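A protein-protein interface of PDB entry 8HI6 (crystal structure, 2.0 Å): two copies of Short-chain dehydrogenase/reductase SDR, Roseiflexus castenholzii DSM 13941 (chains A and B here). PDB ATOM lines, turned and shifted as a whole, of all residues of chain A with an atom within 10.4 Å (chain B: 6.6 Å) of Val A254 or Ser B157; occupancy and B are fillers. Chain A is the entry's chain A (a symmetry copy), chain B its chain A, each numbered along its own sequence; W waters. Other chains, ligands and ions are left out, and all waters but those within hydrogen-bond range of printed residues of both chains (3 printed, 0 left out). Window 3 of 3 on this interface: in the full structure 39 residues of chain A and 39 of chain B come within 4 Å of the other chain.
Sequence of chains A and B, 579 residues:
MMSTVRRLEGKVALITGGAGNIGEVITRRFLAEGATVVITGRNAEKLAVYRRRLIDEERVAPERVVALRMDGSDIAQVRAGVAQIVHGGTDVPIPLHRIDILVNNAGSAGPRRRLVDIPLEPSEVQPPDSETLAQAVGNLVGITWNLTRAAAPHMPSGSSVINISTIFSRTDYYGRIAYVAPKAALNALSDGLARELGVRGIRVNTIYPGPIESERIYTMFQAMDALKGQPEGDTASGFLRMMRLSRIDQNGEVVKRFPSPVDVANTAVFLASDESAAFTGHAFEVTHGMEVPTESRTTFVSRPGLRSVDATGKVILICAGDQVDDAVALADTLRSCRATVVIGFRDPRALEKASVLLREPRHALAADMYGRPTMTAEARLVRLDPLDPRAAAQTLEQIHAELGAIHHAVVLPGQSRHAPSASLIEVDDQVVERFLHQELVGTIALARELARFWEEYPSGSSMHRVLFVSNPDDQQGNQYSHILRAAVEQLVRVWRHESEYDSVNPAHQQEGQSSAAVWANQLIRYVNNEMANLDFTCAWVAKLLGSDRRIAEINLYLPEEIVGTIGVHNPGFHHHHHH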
ATOM      1  N   LEU A 240     -12.076 -33.972   3.205  1.00  0.00           N
ATOM      2  CA  LEU A 240     -11.562 -32.636   3.506  1.00  0.00           C
ATOM      3  C   LEU A 240     -12.632 -31.576   3.274  1.00  0.00           C
ATOM      4  O   LEU A 240     -12.765 -30.634   4.066  1.00  0.00           O
ATOM      5  CB  LEU A 240     -10.316 -32.336   2.650  1.00  0.00           C
ATOM      6  CG  LEU A 240      -9.039 -33.107   3.014  1.00  0.00           C
ATOM      7  CD1 LEU A 240      -7.993 -33.055   1.869  1.00  0.00           C
ATOM      8  CD2 LEU A 240      -8.436 -32.583   4.305  1.00  0.00           C
ATOM      9  N   ARG A 244     -15.700 -28.777   8.764  1.00  0.00           N
ATOM     10  CA  ARG A 244     -16.043 -27.377   8.992  1.00  0.00           C
ATOM     11  C   ARG A 244     -14.886 -26.571   9.563  1.00  0.00           C
ATOM     12  O   ARG A 244     -14.825 -25.351   9.354  1.00  0.00           O
ATOM     13  CB  ARG A 244     -17.240 -27.278   9.945  1.00  0.00           C
ATOM     14  CG  ARG A 244     -18.547 -27.648   9.264  1.00  0.00           C
ATOM     15  CD  ARG A 244     -19.738 -27.386  10.174  1.00  0.00           C
ATOM     16  NE  ARG A 244     -19.817 -28.375  11.237  1.00  0.00           N
ATOM     17  CZ  ARG A 244     -20.733 -28.373  12.195  1.00  0.00           C
ATOM     18  NH1 ARG A 244     -21.645 -27.412  12.281  1.00  0.00           N
ATOM     19  NH2 ARG A 244     -20.731 -29.355  13.091  1.00  0.00           N
ATOM     20  N   LEU A 245     -13.982 -27.208  10.299  1.00  0.00           N
ATOM     21  CA  LEU A 245     -12.905 -26.497  10.979  1.00  0.00           C
ATOM     22  C   LEU A 245     -11.655 -26.541  10.116  1.00  0.00           C
ATOM     23  O   LEU A 245     -11.112 -27.619   9.859  1.00  0.00           O
ATOM     24  CB  LEU A 245     -12.606 -27.095  12.353  1.00  0.00           C
ATOM     25  CG  LEU A 245     -11.534 -26.374  13.179  1.00  0.00           C
ATOM     26  CD1 LEU A 245     -12.000 -24.974  13.598  1.00  0.00           C
ATOM     27  CD2 LEU A 245     -11.189 -27.191  14.401  1.00  0.00           C
ATOM     28  N   SER A 246     -11.223 -25.378   9.653  1.00  0.00           N
ATOM     29  CA  SER A 246      -9.900 -25.235   9.069  1.00  0.00           C
ATOM     30  C   SER A 246      -8.886 -25.030  10.191  1.00  0.00           C
ATOM     31  O   SER A 246      -9.230 -24.619  11.303  1.00  0.00           O
ATOM     32  CB  SER A 246      -9.891 -24.072   8.086  1.00  0.00           C
ATOM     33  OG  SER A 246     -10.685 -24.411   6.963  1.00  0.00           O
ATOM     34  N   ARG A 247      -7.627 -25.361   9.908  1.00  0.00           N
ATOM     35  CA  ARG A 247      -6.677 -25.474  11.004  1.00  0.00           C
ATOM     36  C   ARG A 247      -5.253 -25.276  10.498  1.00  0.00           C
ATOM     37  O   ARG A 247      -4.930 -25.614   9.352  1.00  0.00           O
ATOM     38  CB  ARG A 247      -6.833 -26.833  11.691  1.00  0.00           C
ATOM     39  CG  ARG A 247      -5.960 -27.055  12.886  1.00  0.00           C
ATOM     40  CD  ARG A 247      -6.233 -28.415  13.464  1.00  0.00           C
ATOM     41  NE  ARG A 247      -5.281 -28.746  14.514  1.00  0.00           N
ATOM     42  CZ  ARG A 247      -5.260 -29.903  15.153  1.00  0.00           C
ATOM     43  NH1 ARG A 247      -6.136 -30.857  14.871  1.00  0.00           N
ATOM     44  NH2 ARG A 247      -4.343 -30.112  16.095  1.00  0.00           N
ATOM     45  N   ILE A 248      -4.416 -24.705  11.375  1.00  0.00           N
ATOM     46  CA  ILE A 248      -2.998 -24.493  11.090  1.00  0.00           C
ATOM     47  C   ILE A 248      -2.340 -25.807  10.698  1.00  0.00           C
ATOM     48  O   ILE A 248      -2.390 -26.791  11.446  1.00  0.00           O
ATOM     49  CB  ILE A 248      -2.303 -23.890  12.328  1.00  0.00           C
ATOM     50  CG1 ILE A 248      -2.736 -22.448  12.577  1.00  0.00           C
ATOM     51  CG2 ILE A 248      -0.797 -23.945  12.177  1.00  0.00           C
ATOM     52  CD1 ILE A 248      -2.842 -21.624  11.339  1.00  0.00           C
ATOM     53  N   ASP A 249      -1.703 -25.829   9.529  1.00  0.00           N
ATOM     54  CA  ASP A 249      -0.901 -26.968   9.104  1.00  0.00           C
ATOM     55  C   ASP A 249       0.579 -26.699   9.404  1.00  0.00           C
ATOM     56  O   ASP A 249       0.932 -25.692  10.031  1.00  0.00           O
ATOM     57  CB  ASP A 249      -1.198 -27.267   7.628  1.00  0.00           C
ATOM     58  CG  ASP A 249      -0.476 -26.326   6.667  1.00  0.00           C
ATOM     59  OD1 ASP A 249       0.045 -25.260   7.093  1.00  0.00           O
ATOM     60  OD2 ASP A 249      -0.501 -26.628   5.454  1.00  0.00           O
ATOM     61  N   GLN A 250       1.459 -27.603   8.951  1.00  0.00           N
ATOM     62  CA  GLN A 250       2.883 -27.494   9.278  1.00  0.00           C
ATOM     63  C   GLN A 250       3.508 -26.183   8.806  1.00  0.00           C
ATOM     64  O   GLN A 250       4.508 -25.749   9.382  1.00  0.00           O
ATOM     65  CB  GLN A 250       3.672 -28.659   8.675  1.00  0.00           C
ATOM     66  CG  GLN A 250       3.592 -29.974   9.433  1.00  0.00           C
ATOM     67  CD  GLN A 250       4.112 -31.135   8.590  1.00  0.00           C
ATOM     68  OE1 GLN A 250       5.191 -31.680   8.861  1.00  0.00           O
ATOM     69  NE2 GLN A 250       3.350 -31.518   7.556  1.00  0.00           N
ATOM     70  N   ASN A 251       2.958 -25.548   7.773  1.00  0.00           N
ATOM     71  CA  ASN A 251       3.476 -24.277   7.282  1.00  0.00           C
ATOM     72  C   ASN A 251       2.689 -23.068   7.794  1.00  0.00           C
ATOM     73  O   ASN A 251       2.832 -21.970   7.239  1.00  0.00           O
ATOM     74  CB  ASN A 251       3.508 -24.274   5.750  1.00  0.00           C
ATOM     75  CG  ASN A 251       4.360 -23.141   5.187  1.00  0.00           C
ATOM     76  OD1 ASN A 251       5.383 -22.769   5.765  1.00  0.00           O
ATOM     77  ND2 ASN A 251       3.928 -22.578   4.062  1.00  0.00           N
ATOM     78  N   GLY A 252       1.862 -23.242   8.830  1.00  0.00           N
ATOM     79  CA  GLY A 252       1.138 -22.115   9.395  1.00  0.00           C
ATOM     80  C   GLY A 252      -0.027 -21.606   8.571  1.00  0.00           C
ATOM     81  O   GLY A 252      -0.513 -20.501   8.822  1.00  0.00           O
ATOM     82  N   GLU A 253      -0.501 -22.376   7.595  1.00  0.00           N
ATOM     83  CA  GLU A 253      -1.638 -21.988   6.772  1.00  0.00           C
ATOM     84  C   GLU A 253      -2.925 -22.558   7.358  1.00  0.00           C
ATOM     85  O   GLU A 253      -2.946 -23.707   7.810  1.00  0.00           O
ATOM     86  CB  GLU A 253      -1.442 -22.495   5.345  1.00  0.00           C
ATOM     87  CG  GLU A 253      -2.047 -21.598   4.291  1.00  0.00           C
ATOM     88  CD  GLU A 253      -1.070 -20.526   3.853  1.00  0.00           C
ATOM     89  OE1 GLU A 253      -0.059 -20.330   4.568  1.00  0.00           O
ATOM     90  OE2 GLU A 253      -1.300 -19.893   2.795  1.00  0.00           O
ATOM     91  N   VAL A 254      -3.994 -21.759   7.342  1.00  0.00           N
ATOM     92  CA  VAL A 254      -5.295 -22.191   7.878  1.00  0.00           C
ATOM     93  C   VAL A 254      -6.062 -22.879   6.752  1.00  0.00           C
ATOM     94  O   VAL A 254      -6.640 -22.219   5.882  1.00  0.00           O
ATOM     95  CB  VAL A 254      -6.100 -21.033   8.475  1.00  0.00           C
ATOM     96  CG1 VAL A 254      -7.301 -21.585   9.241  1.00  0.00           C
ATOM     97  CG2 VAL A 254      -5.244 -20.183   9.403  1.00  0.00           C
ATOM     98  N   VAL A 255      -6.084 -24.212   6.776  1.00  0.00           N
ATOM     99  CA  VAL A 255      -6.550 -25.011   5.649  1.00  0.00           C
ATOM    100  C   VAL A 255      -7.356 -26.193   6.171  1.00  0.00           C
ATOM    101  O   VAL A 255      -7.405 -26.456   7.371  1.00  0.00           O
ATOM    102  CB  VAL A 255      -5.370 -25.515   4.799  1.00  0.00           C
ATOM    103  CG1 VAL A 255      -4.624 -24.334   4.171  1.00  0.00           C
ATOM    104  CG2 VAL A 255      -4.449 -26.360   5.670  1.00  0.00           C
ATOM    105  N   LYS A 256      -7.975 -26.922   5.240  1.00  0.00           N
ATOM    106  CA  LYS A 256      -8.490 -28.254   5.536  1.00  0.00           C
ATOM    107  C   LYS A 256      -7.329 -29.240   5.646  1.00  0.00           C
ATOM    108  O   LYS A 256      -6.496 -29.331   4.738  1.00  0.00           O
ATOM    109  CB  LYS A 256      -9.446 -28.718   4.435  1.00  0.00           C
ATOM    110  CG  LYS A 256     -10.604 -27.790   4.145  1.00  0.00           C
ATOM    111  CD  LYS A 256     -11.442 -27.533   5.384  1.00  0.00           C
ATOM    112  CE  LYS A 256     -12.722 -26.777   5.020  1.00  0.00           C
ATOM    113  NZ  LYS A 256     -13.715 -27.666   4.325  1.00  0.00           N
ATOM    114  N   ARG A 257      -7.289 -30.003   6.737  1.00  0.00           N
ATOM    115  CA  ARG A 257      -6.254 -31.012   6.931  1.00  0.00           C
ATOM    116  C   ARG A 257      -6.815 -32.118   7.816  1.00  0.00           C
ATOM    117  O   ARG A 257      -7.861 -31.952   8.449  1.00  0.00           O
ATOM    118  CB  ARG A 257      -5.007 -30.392   7.570  1.00  0.00           C
ATOM    119  CG  ARG A 257      -5.373 -29.450   8.728  1.00  0.00           C
ATOM    120  CD  ARG A 257      -4.277 -29.344   9.776  1.00  0.00           C
ATOM    121  NE  ARG A 257      -4.144 -30.565  10.558  1.00  0.00           N
ATOM    122  CZ  ARG A 257      -3.419 -30.660  11.665  1.00  0.00           C
ATOM    123  NH1 ARG A 257      -2.775 -29.610  12.160  1.00  0.00           N
ATOM    124  NH2 ARG A 257      -3.342 -31.831  12.289  1.00  0.00           N
ATOM    125  N   HIS A 288     -12.721 -32.498  12.988  1.00  0.00           N
ATOM    126  CA  HIS A 288     -12.776 -31.119  12.492  1.00  0.00           C
ATOM    127  C   HIS A 288     -14.198 -30.737  12.087  1.00  0.00           C
ATOM    128  O   HIS A 288     -14.413 -30.016  11.113  1.00  0.00           O
ATOM    129  CB  HIS A 288     -11.807 -30.896  11.322  1.00  0.00           C
ATOM    130  CG  HIS A 288     -10.366 -30.908  11.732  1.00  0.00           C
ATOM    131  ND1 HIS A 288      -9.335 -31.079  10.832  1.00  0.00           N
ATOM    132  CD2 HIS A 288      -9.788 -30.791  12.951  1.00  0.00           C
ATOM    133  CE1 HIS A 288      -8.181 -31.057  11.480  1.00  0.00           C
ATOM    134  NE2 HIS A 288      -8.429 -30.887  12.767  1.00  0.00           N
ATOM    135  N   MET B 155     -10.120 -12.884  17.914  1.00  0.00           N
ATOM    136  CA  MET B 155      -9.742 -14.245  18.250  1.00  0.00           C
ATOM    137  C   MET B 155      -8.926 -14.829  17.109  1.00  0.00           C
ATOM    138  O   MET B 155      -9.462 -14.999  16.001  1.00  0.00           O
ATOM    139  CB  MET B 155     -10.984 -15.089  18.524  1.00  0.00           C
ATOM    140  CG  MET B 155     -11.901 -14.468  19.600  1.00  0.00           C
ATOM    141  SD  MET B 155     -13.338 -15.483  20.020  1.00  0.00           S
ATOM    142  CE  MET B 155     -12.523 -16.831  20.877  1.00  0.00           C
ATOM    143  N   PRO B 156      -7.640 -15.120  17.308  1.00  0.00           N
ATOM    144  CA  PRO B 156      -6.823 -15.679  16.217  1.00  0.00           C
ATOM    145  C   PRO B 156      -7.205 -17.122  15.920  1.00  0.00           C
ATOM    146  O   PRO B 156      -7.915 -17.781  16.678  1.00  0.00           O
ATOM    147  CB  PRO B 156      -5.393 -15.591  16.766  1.00  0.00           C
ATOM    148  CG  PRO B 156      -5.563 -15.642  18.240  1.00  0.00           C
ATOM    149  CD  PRO B 156      -6.856 -14.910  18.539  1.00  0.00           C
ATOM    150  N   SER B 157      -6.699 -17.619  14.794  1.00  0.00           N
ATOM    151  CA  SER B 157      -6.855 -19.026  14.455  1.00  0.00           C
ATOM    152  C   SER B 157      -6.376 -19.907  15.604  1.00  0.00           C
ATOM    153  O   SER B 157      -5.369 -19.614  16.257  1.00  0.00           O
ATOM    154  CB  SER B 157      -6.065 -19.343  13.181  1.00  0.00           C
ATOM    155  OG  SER B 157      -6.399 -20.629  12.660  1.00  0.00           O
ATOM    156  N   GLY B 158      -7.100 -20.996  15.853  1.00  0.00           N
ATOM    157  CA  GLY B 158      -6.813 -21.855  16.988  1.00  0.00           C
ATOM    158  C   GLY B 158      -7.553 -21.498  18.267  1.00  0.00           C
ATOM    159  O   GLY B 158      -7.420 -22.219  19.266  1.00  0.00           O
ATOM    160  N   SER B 159      -8.334 -20.422  18.265  1.00  0.00           N
ATOM    161  CA  SER B 159      -9.074 -19.987  19.440  1.00  0.00           C
ATOM    162  C   SER B 159     -10.327 -20.845  19.642  1.00  0.00           C
ATOM    163  O   SER B 159     -10.742 -21.598  18.756  1.00  0.00           O
ATOM    164  CB  SER B 159      -9.470 -18.523  19.295  1.00  0.00           C
ATOM    165  OG  SER B 159      -8.326 -17.708  19.147  1.00  0.00           O
ATOM    166  N   GLY B 198     -15.489 -21.589  11.538  1.00  0.00           N
ATOM    167  CA  GLY B 198     -14.523 -22.634  11.246  1.00  0.00           C
ATOM    168  C   GLY B 198     -13.544 -22.251  10.154  1.00  0.00           C
ATOM    169  O   GLY B 198     -12.377 -22.643  10.201  1.00  0.00           O
ATOM    170  N   VAL B 199     -13.990 -21.455   9.179  1.00  0.00           N
ATOM    171  CA  VAL B 199     -13.090 -21.032   8.112  1.00  0.00           C
ATOM    172  C   VAL B 199     -11.960 -20.158   8.650  1.00  0.00           C
ATOM    173  O   VAL B 199     -10.885 -20.087   8.038  1.00  0.00           O
ATOM    174  CB  VAL B 199     -13.886 -20.324   6.991  1.00  0.00           C
ATOM    175  CG1 VAL B 199     -14.396 -18.989   7.446  1.00  0.00           C
ATOM    176  CG2 VAL B 199     -13.028 -20.173   5.738  1.00  0.00           C
ATOM    177  N   ARG B 200     -12.155 -19.524   9.808  1.00  0.00           N
ATOM    178  CA  ARG B 200     -11.109 -18.743  10.448  1.00  0.00           C
ATOM    179  C   ARG B 200     -10.267 -19.559  11.414  1.00  0.00           C
ATOM    180  O   ARG B 200      -9.384 -18.998  12.064  1.00  0.00           O
ATOM    181  CB  ARG B 200     -11.714 -17.562  11.206  1.00  0.00           C
ATOM    182  CG  ARG B 200     -12.715 -16.754  10.399  1.00  0.00           C
ATOM    183  CD  ARG B 200     -13.204 -15.578  11.219  1.00  0.00           C
ATOM    184  NE  ARG B 200     -14.394 -14.940  10.668  1.00  0.00           N
ATOM    185  CZ  ARG B 200     -14.938 -13.840  11.172  1.00  0.00           C
ATOM    186  NH1 ARG B 200     -14.398 -13.219  12.210  1.00  0.00           N
ATOM    187  NH2 ARG B 200     -16.044 -13.345  10.617  1.00  0.00           N
ATOM    188  N   GLY B 201     -10.536 -20.851  11.559  1.00  0.00           N
ATOM    189  CA  GLY B 201      -9.836 -21.631  12.561  1.00  0.00           C
ATOM    190  C   GLY B 201     -10.314 -21.437  13.984  1.00  0.00           C
ATOM    191  O   GLY B 201      -9.613 -21.837  14.922  1.00  0.00           O
ATOM    192  N   ILE B 202     -11.477 -20.830  14.186  1.00  0.00           N
ATOM    193  CA  ILE B 202     -12.044 -20.659  15.519  1.00  0.00           C
ATOM    194  C   ILE B 202     -13.038 -21.787  15.747  1.00  0.00           C
ATOM    195  O   ILE B 202     -14.008 -21.923  14.998  1.00  0.00           O
ATOM    196  CB  ILE B 202     -12.734 -19.295  15.673  1.00  0.00           C
ATOM    197  CG1 ILE B 202     -11.752 -18.149  15.385  1.00  0.00           C
ATOM    198  CG2 ILE B 202     -13.322 -19.187  17.073  1.00  0.00           C
ATOM    199  CD1 ILE B 202     -12.404 -16.795  15.203  1.00  0.00           C
ATOM    200  N   ARG B 203     -12.828 -22.593  16.774  1.00  0.00           N
ATOM    201  CA  ARG B 203     -13.790 -23.655  17.018  1.00  0.00           C
ATOM    202  C   ARG B 203     -14.869 -23.201  18.005  1.00  0.00           C
ATOM    203  O   ARG B 203     -14.648 -22.327  18.853  1.00  0.00           O
ATOM    204  CB  ARG B 203     -13.083 -24.921  17.504  1.00  0.00           C
ATOM    205  CG  ARG B 203     -12.325 -24.826  18.825  1.00  0.00           C
ATOM    206  CD  ARG B 203     -11.227 -25.911  18.840  1.00  0.00           C
ATOM    207  NE  ARG B 203     -10.547 -25.992  20.131  1.00  0.00           N
ATOM    208  CZ  ARG B 203      -9.498 -25.258  20.454  1.00  0.00           C
ATOM    209  NH1 ARG B 203      -8.973 -24.393  19.600  1.00  0.00           N
ATOM    210  NH2 ARG B 203      -8.966 -25.387  21.664  1.00  0.00           N
HETATM  211  O   HOH W   1      -9.350 -21.004   5.921  1.00  0.00           O
HETATM  212  O   HOH W   2      -8.268 -24.369  13.855  1.00  0.00           O
HETATM  213  O   HOH W   3      -5.625 -23.333  13.925  1.00  0.00           O
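Val A254 touches one residue of chain B. Of chain A, only Ile A248 (3.9 Å) and Val A254 (3.5 Å) come within 4 Å of Ser B157. Pro B156 touches none of the printed residues of chain A. No residue of chain A comes within 4 Å of Ser B159. Of chain A, only Leu A245 (3.9 Å) and Ser A246 (3.3 Å) come within 4 Å of Gly B201. Printed residues of chain B within 4 Å of Ile A248: Ser B157 (3.9 Å). Of the printed residues of chain B, Leu A245 touches Gly B198 (3.97 Å), Gly B201 (3.9 Å) and Ile B202 (3.9 Å). The nearest printed residue of chain A that does not touch Gly B198 is Val A254 (5.3 Å).
N of Leu A245 sits at hydrogen-bond distance from O of His A288, at 3.0 Å. The backbone carbonyl oxygen (O) of Arg B200 sits at hydrogen-bond distance from the side-chain hydroxyl (OG) of Ser B157 (3.5 Å). O of His A288 is in hydrogen-bond range of N of Arg A244 (3.0 Å). The backbone carbonyl oxygen of Gly B201 is in hydrogen-bond range of the backbone NH of Gly B158 (2.8 Å). The guanidinium group (NH1) of Arg A257 sits at hydrogen-bond distance from the backbone carbonyl oxygen (O) of Ile A248 (2.9 Å).
Of the 11 printed residues of chain B, 5 touch a printed residue of chain A. Printed residues of chain B that touch a printed residue of chain A: Ser B157, Gly B198, Val B199, Gly B201 and Ile B202. Along chain B the printed residues that touch a printed residue of chain A span positions 157 to 202. Of the 16 printed residues of chain A, 5 touch a printed residue of chain B. Hydrophobic or aromatic side chains of chain A that line the printed part of chain B: Leu A245, Ile A248 and Val A254. Among the printed residues, no Asp or Glu carboxylate lies within 4 Å of a Lys or Arg side-chain nitrogen of the other chain.
Among the printed residues, merely in contact across the chains: Ser A246 with Gly B201, Arg A244 with Gly B198, Val A254 with Ser B157, Leu A245 with Ile B202, Ile A248 with Ser B157, Leu A245 with Gly B201, Leu A245 with Gly B198 and Arg A244 with Val B199.
No position is printed for both chains.
The backbone carbonyl oxygen (O) of Gly B198 is in hydrogen-bond range of the backbone NH (N) of Ser A246.
Water W2 bridges the backbone carbonyl oxygen of Ser A246 and the backbone carbonyl oxygen of Gly B201. Water W1 lies within hydrogen-bond range of the backbone carbonyl oxygen of Val B199 (2.8 Å) and the backbone carbonyl oxygen of Val A254 (3.0 Å). Water W3 lies within hydrogen-bond range of the side-chain hydroxyl (OG) of Ser B157, the backbone NH (N) of Ile A248 and the backbone NH (N) of Gly B158.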
